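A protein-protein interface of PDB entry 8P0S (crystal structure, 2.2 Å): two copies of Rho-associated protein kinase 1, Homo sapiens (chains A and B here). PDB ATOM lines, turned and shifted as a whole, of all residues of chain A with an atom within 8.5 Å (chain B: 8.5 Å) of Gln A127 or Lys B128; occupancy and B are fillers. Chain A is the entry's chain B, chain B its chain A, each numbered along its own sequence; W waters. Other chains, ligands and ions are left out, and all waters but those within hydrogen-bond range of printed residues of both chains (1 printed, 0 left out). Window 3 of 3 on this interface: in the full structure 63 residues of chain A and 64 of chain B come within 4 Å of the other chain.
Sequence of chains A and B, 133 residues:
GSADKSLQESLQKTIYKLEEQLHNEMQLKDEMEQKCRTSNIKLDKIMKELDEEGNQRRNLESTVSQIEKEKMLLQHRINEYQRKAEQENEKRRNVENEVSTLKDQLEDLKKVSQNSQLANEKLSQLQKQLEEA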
ATOM      1  N   ASN A 120      20.927   3.541  31.533  1.00  0.00           N
ATOM      2  CA  ASN A 120      20.184   4.312  30.543  1.00  0.00           C
ATOM      3  C   ASN A 120      20.453   5.804  30.656  1.00  0.00           C
ATOM      4  O   ASN A 120      20.326   6.523  29.660  1.00  0.00           O
ATOM      5  CB  ASN A 120      18.685   4.036  30.650  1.00  0.00           C
ATOM      6  CG  ASN A 120      18.304   2.641  30.162  1.00  0.00           C
ATOM      7  OD1 ASN A 120      19.152   1.868  29.721  1.00  0.00           O
ATOM      8  ND2 ASN A 120      17.028   2.310  30.259  1.00  0.00           N
ATOM      9  N   GLU A 121      20.813   6.296  31.842  1.00  0.00           N
ATOM     10  CA  GLU A 121      21.190   7.703  31.926  1.00  0.00           C
ATOM     11  C   GLU A 121      22.494   7.961  31.168  1.00  0.00           C
ATOM     12  O   GLU A 121      22.640   8.994  30.510  1.00  0.00           O
ATOM     13  CB  GLU A 121      21.303   8.144  33.394  1.00  0.00           C
ATOM     14  CG  GLU A 121      22.442   9.140  33.675  1.00  0.00           C
ATOM     15  CD  GLU A 121      22.690   9.393  35.168  1.00  0.00           C
ATOM     16  OE1 GLU A 121      21.694   9.518  35.923  1.00  0.00           O
ATOM     17  OE2 GLU A 121      23.881   9.477  35.578  1.00  0.00           O
ATOM     18  N   LYS A 122      23.453   7.031  31.233  1.00  0.00           N
ATOM     19  CA  LYS A 122      24.699   7.239  30.496  1.00  0.00           C
ATOM     20  C   LYS A 122      24.487   7.158  28.987  1.00  0.00           C
ATOM     21  O   LYS A 122      25.150   7.884  28.240  1.00  0.00           O
ATOM     22  CB  LYS A 122      25.762   6.230  30.939  1.00  0.00           C
ATOM     23  CG  LYS A 122      26.103   6.299  32.426  1.00  0.00           C
ATOM     24  CD  LYS A 122      26.947   7.509  32.744  1.00  0.00           C
ATOM     25  CE  LYS A 122      27.995   7.165  33.795  1.00  0.00           C
ATOM     26  NZ  LYS A 122      28.689   8.414  34.224  1.00  0.00           N
ATOM     27  N   LEU A 123      23.573   6.301  28.509  1.00  0.00           N
ATOM     28  CA  LEU A 123      23.339   6.242  27.064  1.00  0.00           C
ATOM     29  C   LEU A 123      22.622   7.485  26.573  1.00  0.00           C
ATOM     30  O   LEU A 123      22.937   7.995  25.490  1.00  0.00           O
ATOM     31  CB  LEU A 123      22.556   4.995  26.670  1.00  0.00           C
ATOM     32  CG  LEU A 123      23.298   3.672  26.687  1.00  0.00           C
ATOM     33  CD1 LEU A 123      22.298   2.540  26.458  1.00  0.00           C
ATOM     34  CD2 LEU A 123      24.415   3.623  25.628  1.00  0.00           C
ATOM     35  N   SER A 124      21.665   7.993  27.363  1.00  0.00           N
ATOM     36  CA  SER A 124      21.007   9.261  27.054  1.00  0.00           C
ATOM     37  C   SER A 124      22.014  10.395  26.937  1.00  0.00           C
ATOM     38  O   SER A 124      21.921  11.231  26.030  1.00  0.00           O
ATOM     39  CB  SER A 124      19.993   9.602  28.145  1.00  0.00           C
ATOM     40  OG  SER A 124      18.894   8.716  28.108  1.00  0.00           O
ATOM     41  N   GLN A 125      22.955  10.467  27.883  1.00  0.00           N
ATOM     42  CA  GLN A 125      24.036  11.443  27.789  1.00  0.00           C
ATOM     43  C   GLN A 125      24.908  11.173  26.566  1.00  0.00           C
ATOM     44  O   GLN A 125      25.262  12.110  25.843  1.00  0.00           O
ATOM     45  CB  GLN A 125      24.890  11.429  29.064  1.00  0.00           C
ATOM     46  CG  GLN A 125      24.269  12.214  30.230  1.00  0.00           C
ATOM     47  CD  GLN A 125      25.083  12.127  31.521  1.00  0.00           C
ATOM     48  OE1 GLN A 125      24.562  11.746  32.582  1.00  0.00           O
ATOM     49  NE2 GLN A 125      26.361  12.508  31.442  1.00  0.00           N
ATOM     50  N   LEU A 126      25.270   9.901  26.328  1.00  0.00           N
ATOM     51  CA  LEU A 126      26.046   9.570  25.131  1.00  0.00           C
ATOM     52  C   LEU A 126      25.334  10.054  23.875  1.00  0.00           C
ATOM     53  O   LEU A 126      25.931  10.733  23.033  1.00  0.00           O
ATOM     54  CB  LEU A 126      26.328   8.069  25.050  1.00  0.00           C
ATOM     55  CG  LEU A 126      27.011   7.681  23.738  1.00  0.00           C
ATOM     56  CD1 LEU A 126      28.296   8.450  23.669  1.00  0.00           C
ATOM     57  CD2 LEU A 126      27.308   6.191  23.666  1.00  0.00           C
ATOM     58  N   GLN A 127      24.035   9.776  23.769  1.00  0.00           N
ATOM     59  CA  GLN A 127      23.290  10.211  22.594  1.00  0.00           C
ATOM     60  C   GLN A 127      23.304  11.724  22.457  1.00  0.00           C
ATOM     61  O   GLN A 127      23.326  12.261  21.341  1.00  0.00           O
ATOM     62  CB  GLN A 127      21.860   9.702  22.677  1.00  0.00           C
ATOM     63  CG  GLN A 127      21.071   9.924  21.400  1.00  0.00           C
ATOM     64  CD  GLN A 127      19.685   9.338  21.500  1.00  0.00           C
ATOM     65  OE1 GLN A 127      19.473   8.364  22.235  1.00  0.00           O
ATOM     66  NE2 GLN A 127      18.726   9.918  20.761  1.00  0.00           N
ATOM     67  N   LYS A 128      23.245  12.432  23.579  1.00  0.00           N
ATOM     68  CA  LYS A 128      23.268  13.885  23.509  1.00  0.00           C
ATOM     69  C   LYS A 128      24.607  14.371  22.971  1.00  0.00           C
ATOM     70  O   LYS A 128      24.658  15.276  22.133  1.00  0.00           O
ATOM     71  CB  LYS A 128      22.993  14.475  24.896  1.00  0.00           C
ATOM     72  CG  LYS A 128      23.237  15.975  24.999  1.00  0.00           C
ATOM     73  CD  LYS A 128      21.991  16.753  24.579  1.00  0.00           C
ATOM     74  CE  LYS A 128      22.270  18.245  24.474  1.00  0.00           C
ATOM     75  NZ  LYS A 128      21.278  18.911  23.587  1.00  0.00           N
ATOM     76  N   GLN A 129      25.700  13.755  23.425  1.00  0.00           N
ATOM     77  CA  GLN A 129      27.010  14.219  22.994  1.00  0.00           C
ATOM     78  C   GLN A 129      27.334  13.825  21.562  1.00  0.00           C
ATOM     79  O   GLN A 129      28.244  14.418  20.967  1.00  0.00           O
ATOM     80  CB  GLN A 129      28.082  13.692  23.933  1.00  0.00           C
ATOM     81  CG  GLN A 129      28.126  14.472  25.210  1.00  0.00           C
ATOM     82  CD  GLN A 129      28.864  13.741  26.270  1.00  0.00           C
ATOM     83  OE1 GLN A 129      28.719  12.534  26.399  1.00  0.00           O
ATOM     84  NE2 GLN A 129      29.647  14.460  27.052  1.00  0.00           N
ATOM     85  N   LEU A 130      26.605  12.879  20.980  1.00  0.00           N
ATOM     86  CA  LEU A 130      26.820  12.487  19.600  1.00  0.00           C
ATOM     87  C   LEU A 130      25.927  13.250  18.634  1.00  0.00           C
ATOM     88  O   LEU A 130      26.029  13.032  17.426  1.00  0.00           O
ATOM     89  CB  LEU A 130      26.601  10.970  19.441  1.00  0.00           C
ATOM     90  CG  LEU A 130      27.629  10.053  20.132  1.00  0.00           C
ATOM     91  CD1 LEU A 130      27.426   8.585  19.793  1.00  0.00           C
ATOM     92  CD2 LEU A 130      29.050  10.462  19.855  1.00  0.00           C
ATOM     93  N   GLU A 131      25.078  14.152  19.124  1.00  0.00           N
ATOM     94  CA  GLU A 131      24.129  14.828  18.244  1.00  0.00           C
ATOM     95  C   GLU A 131      24.821  15.901  17.400  1.00  0.00           C
ATOM     96  O   GLU A 131      25.853  16.460  17.781  1.00  0.00           O
ATOM     97  CB  GLU A 131      22.978  15.417  19.061  1.00  0.00           C
ATOM     98  CG  GLU A 131      23.294  16.739  19.740  1.00  0.00           C
ATOM     99  CD  GLU A 131      22.094  17.682  19.853  1.00  0.00           C
ATOM    100  OE1 GLU A 131      21.000  17.238  20.324  1.00  0.00           O
ATOM    101  OE2 GLU A 131      22.274  18.877  19.496  1.00  0.00           O
ATOM    102  N   GLU A 132      24.252  16.167  16.224  1.00  0.00           N
ATOM    103  CA  GLU A 132      24.896  17.023  15.221  1.00  0.00           C
ATOM    104  C   GLU A 132      24.372  18.456  15.267  1.00  0.00           C
ATOM    105  O   GLU A 132      23.817  18.957  14.289  1.00  0.00           O
ATOM    106  CB  GLU A 132      24.719  16.435  13.824  1.00  0.00           C
ATOM    107  CG  GLU A 132      25.180  14.989  13.687  1.00  0.00           C
ATOM    108  CD  GLU A 132      25.504  14.626  12.240  1.00  0.00           C
ATOM    109  OE1 GLU A 132      24.608  14.791  11.374  1.00  0.00           O
ATOM    110  OE2 GLU A 132      26.656  14.198  11.971  1.00  0.00           O
ATOM    111  N   ASN B 120      12.351   4.460  28.330  1.00  0.00           N
ATOM    112  CA  ASN B 120      13.648   5.015  27.964  1.00  0.00           C
ATOM    113  C   ASN B 120      13.914   4.885  26.473  1.00  0.00           C
ATOM    114  O   ASN B 120      14.435   5.819  25.851  1.00  0.00           O
ATOM    115  CB  ASN B 120      14.742   4.331  28.768  1.00  0.00           C
ATOM    116  CG  ASN B 120      15.095   5.109  29.996  1.00  0.00           C
ATOM    117  OD1 ASN B 120      14.891   4.644  31.121  1.00  0.00           O
ATOM    118  ND2 ASN B 120      15.642   6.308  29.796  1.00  0.00           N
ATOM    119  N   GLU B 121      13.548   3.745  25.883  1.00  0.00           N
ATOM    120  CA  GLU B 121      13.760   3.574  24.449  1.00  0.00           C
ATOM    121  C   GLU B 121      12.865   4.510  23.636  1.00  0.00           C
ATOM    122  O   GLU B 121      13.326   5.115  22.659  1.00  0.00           O
ATOM    123  CB  GLU B 121      13.557   2.108  24.053  1.00  0.00           C
ATOM    124  CG  GLU B 121      14.684   1.188  24.562  1.00  0.00           C
ATOM    125  CD  GLU B 121      14.284  -0.296  24.670  1.00  0.00           C
ATOM    126  OE1 GLU B 121      13.311  -0.628  25.393  1.00  0.00           O
ATOM    127  OE2 GLU B 121      14.967  -1.139  24.046  1.00  0.00           O
ATOM    128  N   LYS B 122      11.604   4.691  24.034  1.00  0.00           N
ATOM    129  CA  LYS B 122      10.784   5.665  23.321  1.00  0.00           C
ATOM    130  C   LYS B 122      11.396   7.057  23.433  1.00  0.00           C
ATOM    131  O   LYS B 122      11.509   7.788  22.440  1.00  0.00           O
ATOM    132  CB  LYS B 122       9.352   5.675  23.852  1.00  0.00           C
ATOM    133  CG  LYS B 122       8.448   6.641  23.050  1.00  0.00           C
ATOM    134  CD  LYS B 122       7.509   7.479  23.921  1.00  0.00           C
ATOM    135  CE  LYS B 122       6.085   7.500  23.361  1.00  0.00           C
ATOM    136  NZ  LYS B 122       5.169   8.384  24.160  1.00  0.00           N
ATOM    137  N   LEU B 123      11.815   7.427  24.642  1.00  0.00           N
ATOM    138  CA  LEU B 123      12.390   8.745  24.880  1.00  0.00           C
ATOM    139  C   LEU B 123      13.658   8.944  24.057  1.00  0.00           C
ATOM    140  O   LEU B 123      13.870  10.019  23.482  1.00  0.00           O
ATOM    141  CB  LEU B 123      12.662   8.893  26.373  1.00  0.00           C
ATOM    142  CG  LEU B 123      12.876  10.202  27.086  1.00  0.00           C
ATOM    143  CD1 LEU B 123      11.962  10.216  28.300  1.00  0.00           C
ATOM    144  CD2 LEU B 123      14.337  10.242  27.514  1.00  0.00           C
ATOM    145  N   SER B 124      14.497   7.906  23.950  1.00  0.00           N
ATOM    146  CA  SER B 124      15.671   8.007  23.086  1.00  0.00           C
ATOM    147  C   SER B 124      15.290   8.215  21.621  1.00  0.00           C
ATOM    148  O   SER B 124      16.004   8.908  20.881  1.00  0.00           O
ATOM    149  CB  SER B 124      16.533   6.760  23.219  1.00  0.00           C
ATOM    150  OG  SER B 124      17.353   6.630  22.071  1.00  0.00           O
ATOM    151  N   GLN B 125      14.174   7.626  21.176  1.00  0.00           N
ATOM    152  CA  GLN B 125      13.751   7.825  19.789  1.00  0.00           C
ATOM    153  C   GLN B 125      13.202   9.227  19.564  1.00  0.00           C
ATOM    154  O   GLN B 125      13.415   9.807  18.496  1.00  0.00           O
ATOM    155  CB  GLN B 125      12.712   6.784  19.392  1.00  0.00           C
ATOM    156  CG  GLN B 125      13.317   5.445  19.039  1.00  0.00           C
ATOM    157  CD  GLN B 125      12.351   4.311  19.288  1.00  0.00           C
ATOM    158  OE1 GLN B 125      12.716   3.284  19.870  1.00  0.00           O
ATOM    159  NE2 GLN B 125      11.105   4.486  18.839  1.00  0.00           N
ATOM    160  N   LEU B 126      12.493   9.783  20.559  1.00  0.00           N
ATOM    161  CA  LEU B 126      12.022  11.162  20.466  1.00  0.00           C
ATOM    162  C   LEU B 126      13.180  12.155  20.506  1.00  0.00           C
ATOM    163  O   LEU B 126      13.167  13.128  19.745  1.00  0.00           O
ATOM    164  CB  LEU B 126      11.008  11.474  21.574  1.00  0.00           C
ATOM    165  CG  LEU B 126       9.662  10.720  21.554  1.00  0.00           C
ATOM    166  CD1 LEU B 126       8.996  10.780  22.930  1.00  0.00           C
ATOM    167  CD2 LEU B 126       8.723  11.261  20.444  1.00  0.00           C
ATOM    168  N   GLN B 127      14.184  11.947  21.385  1.00  0.00           N
ATOM    169  CA  GLN B 127      15.363  12.825  21.346  1.00  0.00           C
ATOM    170  C   GLN B 127      15.961  12.835  19.950  1.00  0.00           C
ATOM    171  O   GLN B 127      16.421  13.876  19.467  1.00  0.00           O
ATOM    172  CB  GLN B 127      16.468  12.399  22.318  1.00  0.00           C
ATOM    173  CG  GLN B 127      16.185  12.418  23.810  1.00  0.00           C
ATOM    174  CD  GLN B 127      17.184  11.525  24.587  1.00  0.00           C
ATOM    175  OE1 GLN B 127      16.788  10.696  25.420  1.00  0.00           O
ATOM    176  NE2 GLN B 127      18.485  11.692  24.301  1.00  0.00           N
ATOM    177  N   LYS B 128      15.971  11.666  19.297  1.00  0.00           N
ATOM    178  CA  LYS B 128      16.484  11.560  17.936  1.00  0.00           C
ATOM    179  C   LYS B 128      15.631  12.361  16.957  1.00  0.00           C
ATOM    180  O   LYS B 128      16.172  13.046  16.082  1.00  0.00           O
ATOM    181  CB  LYS B 128      16.550  10.089  17.517  1.00  0.00           C
ATOM    182  CG  LYS B 128      17.336   9.846  16.230  1.00  0.00           C
ATOM    183  CD  LYS B 128      18.779  10.326  16.423  1.00  0.00           C
ATOM    184  CE  LYS B 128      19.736   9.740  15.391  1.00  0.00           C
ATOM    185  NZ  LYS B 128      21.129  10.261  15.599  1.00  0.00           N
ATOM    186  N   GLN B 129      14.297  12.290  17.086  1.00  0.00           N
ATOM    187  CA  GLN B 129      13.446  13.077  16.192  1.00  0.00           C
ATOM    188  C   GLN B 129      13.651  14.573  16.425  1.00  0.00           C
ATOM    189  O   GLN B 129      13.645  15.360  15.466  1.00  0.00           O
ATOM    190  CB  GLN B 129      11.968  12.683  16.359  1.00  0.00           C
ATOM    191  CG  GLN B 129      11.614  11.253  15.920  1.00  0.00           C
ATOM    192  CD  GLN B 129      10.117  10.902  16.068  1.00  0.00           C
ATOM    193  OE1 GLN B 129       9.527  11.020  17.144  1.00  0.00           O
ATOM    194  NE2 GLN B 129       9.507  10.473  14.969  1.00  0.00           N
ATOM    195  N   LEU B 130      13.863  14.982  17.689  1.00  0.00           N
ATOM    196  CA  LEU B 130      14.211  16.376  17.970  1.00  0.00           C
ATOM    197  C   LEU B 130      15.510  16.770  17.260  1.00  0.00           C
ATOM    198  O   LEU B 130      15.561  17.787  16.563  1.00  0.00           O
ATOM    199  CB  LEU B 130      14.333  16.623  19.486  1.00  0.00           C
ATOM    200  CG  LEU B 130      14.553  18.118  19.860  1.00  0.00           C
ATOM    201  CD1 LEU B 130      13.688  19.074  19.015  1.00  0.00           C
ATOM    202  CD2 LEU B 130      14.375  18.445  21.368  1.00  0.00           C
ATOM    203  N   GLU B 131      16.576  15.974  17.434  1.00  0.00           N
ATOM    204  CA  GLU B 131      17.857  16.305  16.807  1.00  0.00           C
ATOM    205  C   GLU B 131      17.704  16.482  15.299  1.00  0.00           C
ATOM    206  O   GLU B 131      18.298  17.390  14.702  1.00  0.00           O
ATOM    207  CB  GLU B 131      18.905  15.217  17.099  1.00  0.00           C
ATOM    208  CG  GLU B 131      20.220  15.415  16.306  1.00  0.00           C
ATOM    209  CD  GLU B 131      21.152  14.197  16.289  1.00  0.00           C
ATOM    210  OE1 GLU B 131      20.983  13.240  17.086  1.00  0.00           O
ATOM    211  OE2 GLU B 131      22.080  14.212  15.457  1.00  0.00           O
ATOM    212  N   GLU B 132      16.894  15.630  14.668  1.00  0.00           N
ATOM    213  CA  GLU B 132      16.839  15.599  13.215  1.00  0.00           C
ATOM    214  C   GLU B 132      15.893  16.644  12.634  1.00  0.00           C
ATOM    215  O   GLU B 132      15.996  16.947  11.442  1.00  0.00           O
ATOM    216  CB  GLU B 132      16.449  14.192  12.750  1.00  0.00           C
ATOM    217  CG  GLU B 132      17.445  13.122  13.186  1.00  0.00           C
ATOM    218  CD  GLU B 132      17.085  11.731  12.685  1.00  0.00           C
ATOM    219  OE1 GLU B 132      17.996  10.868  12.595  1.00  0.00           O
ATOM    220  OE2 GLU B 132      15.884  11.498  12.398  1.00  0.00           O
ATOM    221  N   ALA B 133      14.993  17.210  13.437  1.00  0.00           N
ATOM    222  CA  ALA B 133      14.061  18.223  12.943  1.00  0.00           C
ATOM    223  C   ALA B 133      14.716  19.596  12.914  1.00  0.00           C
ATOM    224  O   ALA B 133      15.476  19.910  12.001  1.00  0.00           O
ATOM    225  CB  ALA B 133      12.814  18.260  13.796  1.00  0.00           C
HETATM  226  O   HOH W   1      19.561  12.461  19.572  1.00  0.00           O
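The side-chain amide oxygen (OD1) of Asn B120 lies within hydrogen-bond range of the side-chain amide nitrogen (ND2) of Asn A120 (3.3 Å). OE1 of Gln A127 lies within hydrogen-bond range of OG of Ser B124 (2.7 Å). OE2 of Glu B131 lies within hydrogen-bond range of N of Glu A132 (3.0 Å).
OE1 of Glu B131 is in salt-bridge range of NZ of Lys B128 (3.3 Å). OG of Ser A124 lies within hydrogen-bond range of O of Asn A120 (3.0 Å). OE1 of Glu A131 is in salt-bridge range of NZ of Lys A128 (3.7 Å).
Ser A124 touches Gln B127 (O to NE2, 3.9 Å). Gln B127 touches Gln A127 (CB to NE2, 3.7 Å). Gln A127 touches Lys B128. OE2 of Glu B131 touches CA of Glu A131, 3.5 Å away.
Leu A126 touches none of the printed residues of chain B. Printed residues of chain B within 4 Å of Glu A131: Glu B131 (3.5 Å). Printed residues of chain A within 4 Å of Ser B124: Gln A127 (2.7 Å). Printed residues of chain A within 4 Å of Gln B127: Ser A124 and Gln A127. Of chain A, only Gln A127 (3.6 Å) comes within 4 Å of Lys B128. Gln B129 touches none of the printed residues of chain A. The nearest residue of chain A that does not touch Lys B128 is Leu A130 (5.9 Å).
Printed residues of chain A that touch a printed residue of chain B: Asn A120, Ser A124, Gln A127, Glu A131 and Glu A132. Among the printed residues, no Asp or Glu carboxylate lies within 4 Å of a Lys or Arg side-chain nitrogen of the other chain.
Asn A120 touches its own counterpart, Asn B120. Ser A124 touches Gln B127, and with the chains exchanged Gln A127 touches Ser B124. Gln A127 touches Lys B128, but with the chains exchanged Lys A128 does not touch Gln B127 (4.9 Å). Glu B131 touches its own counterpart, Glu A131. Of the 7 pairs that touch across the chains among the printed residues, 5 have their exchanged pair printed and touching as well.
Water W1 lies within hydrogen-bond range of NE2 of Gln A127 (2.9 Å), OE1 of Glu B131 (3.0 Å) and O of Gln B127 (3.4 Å).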
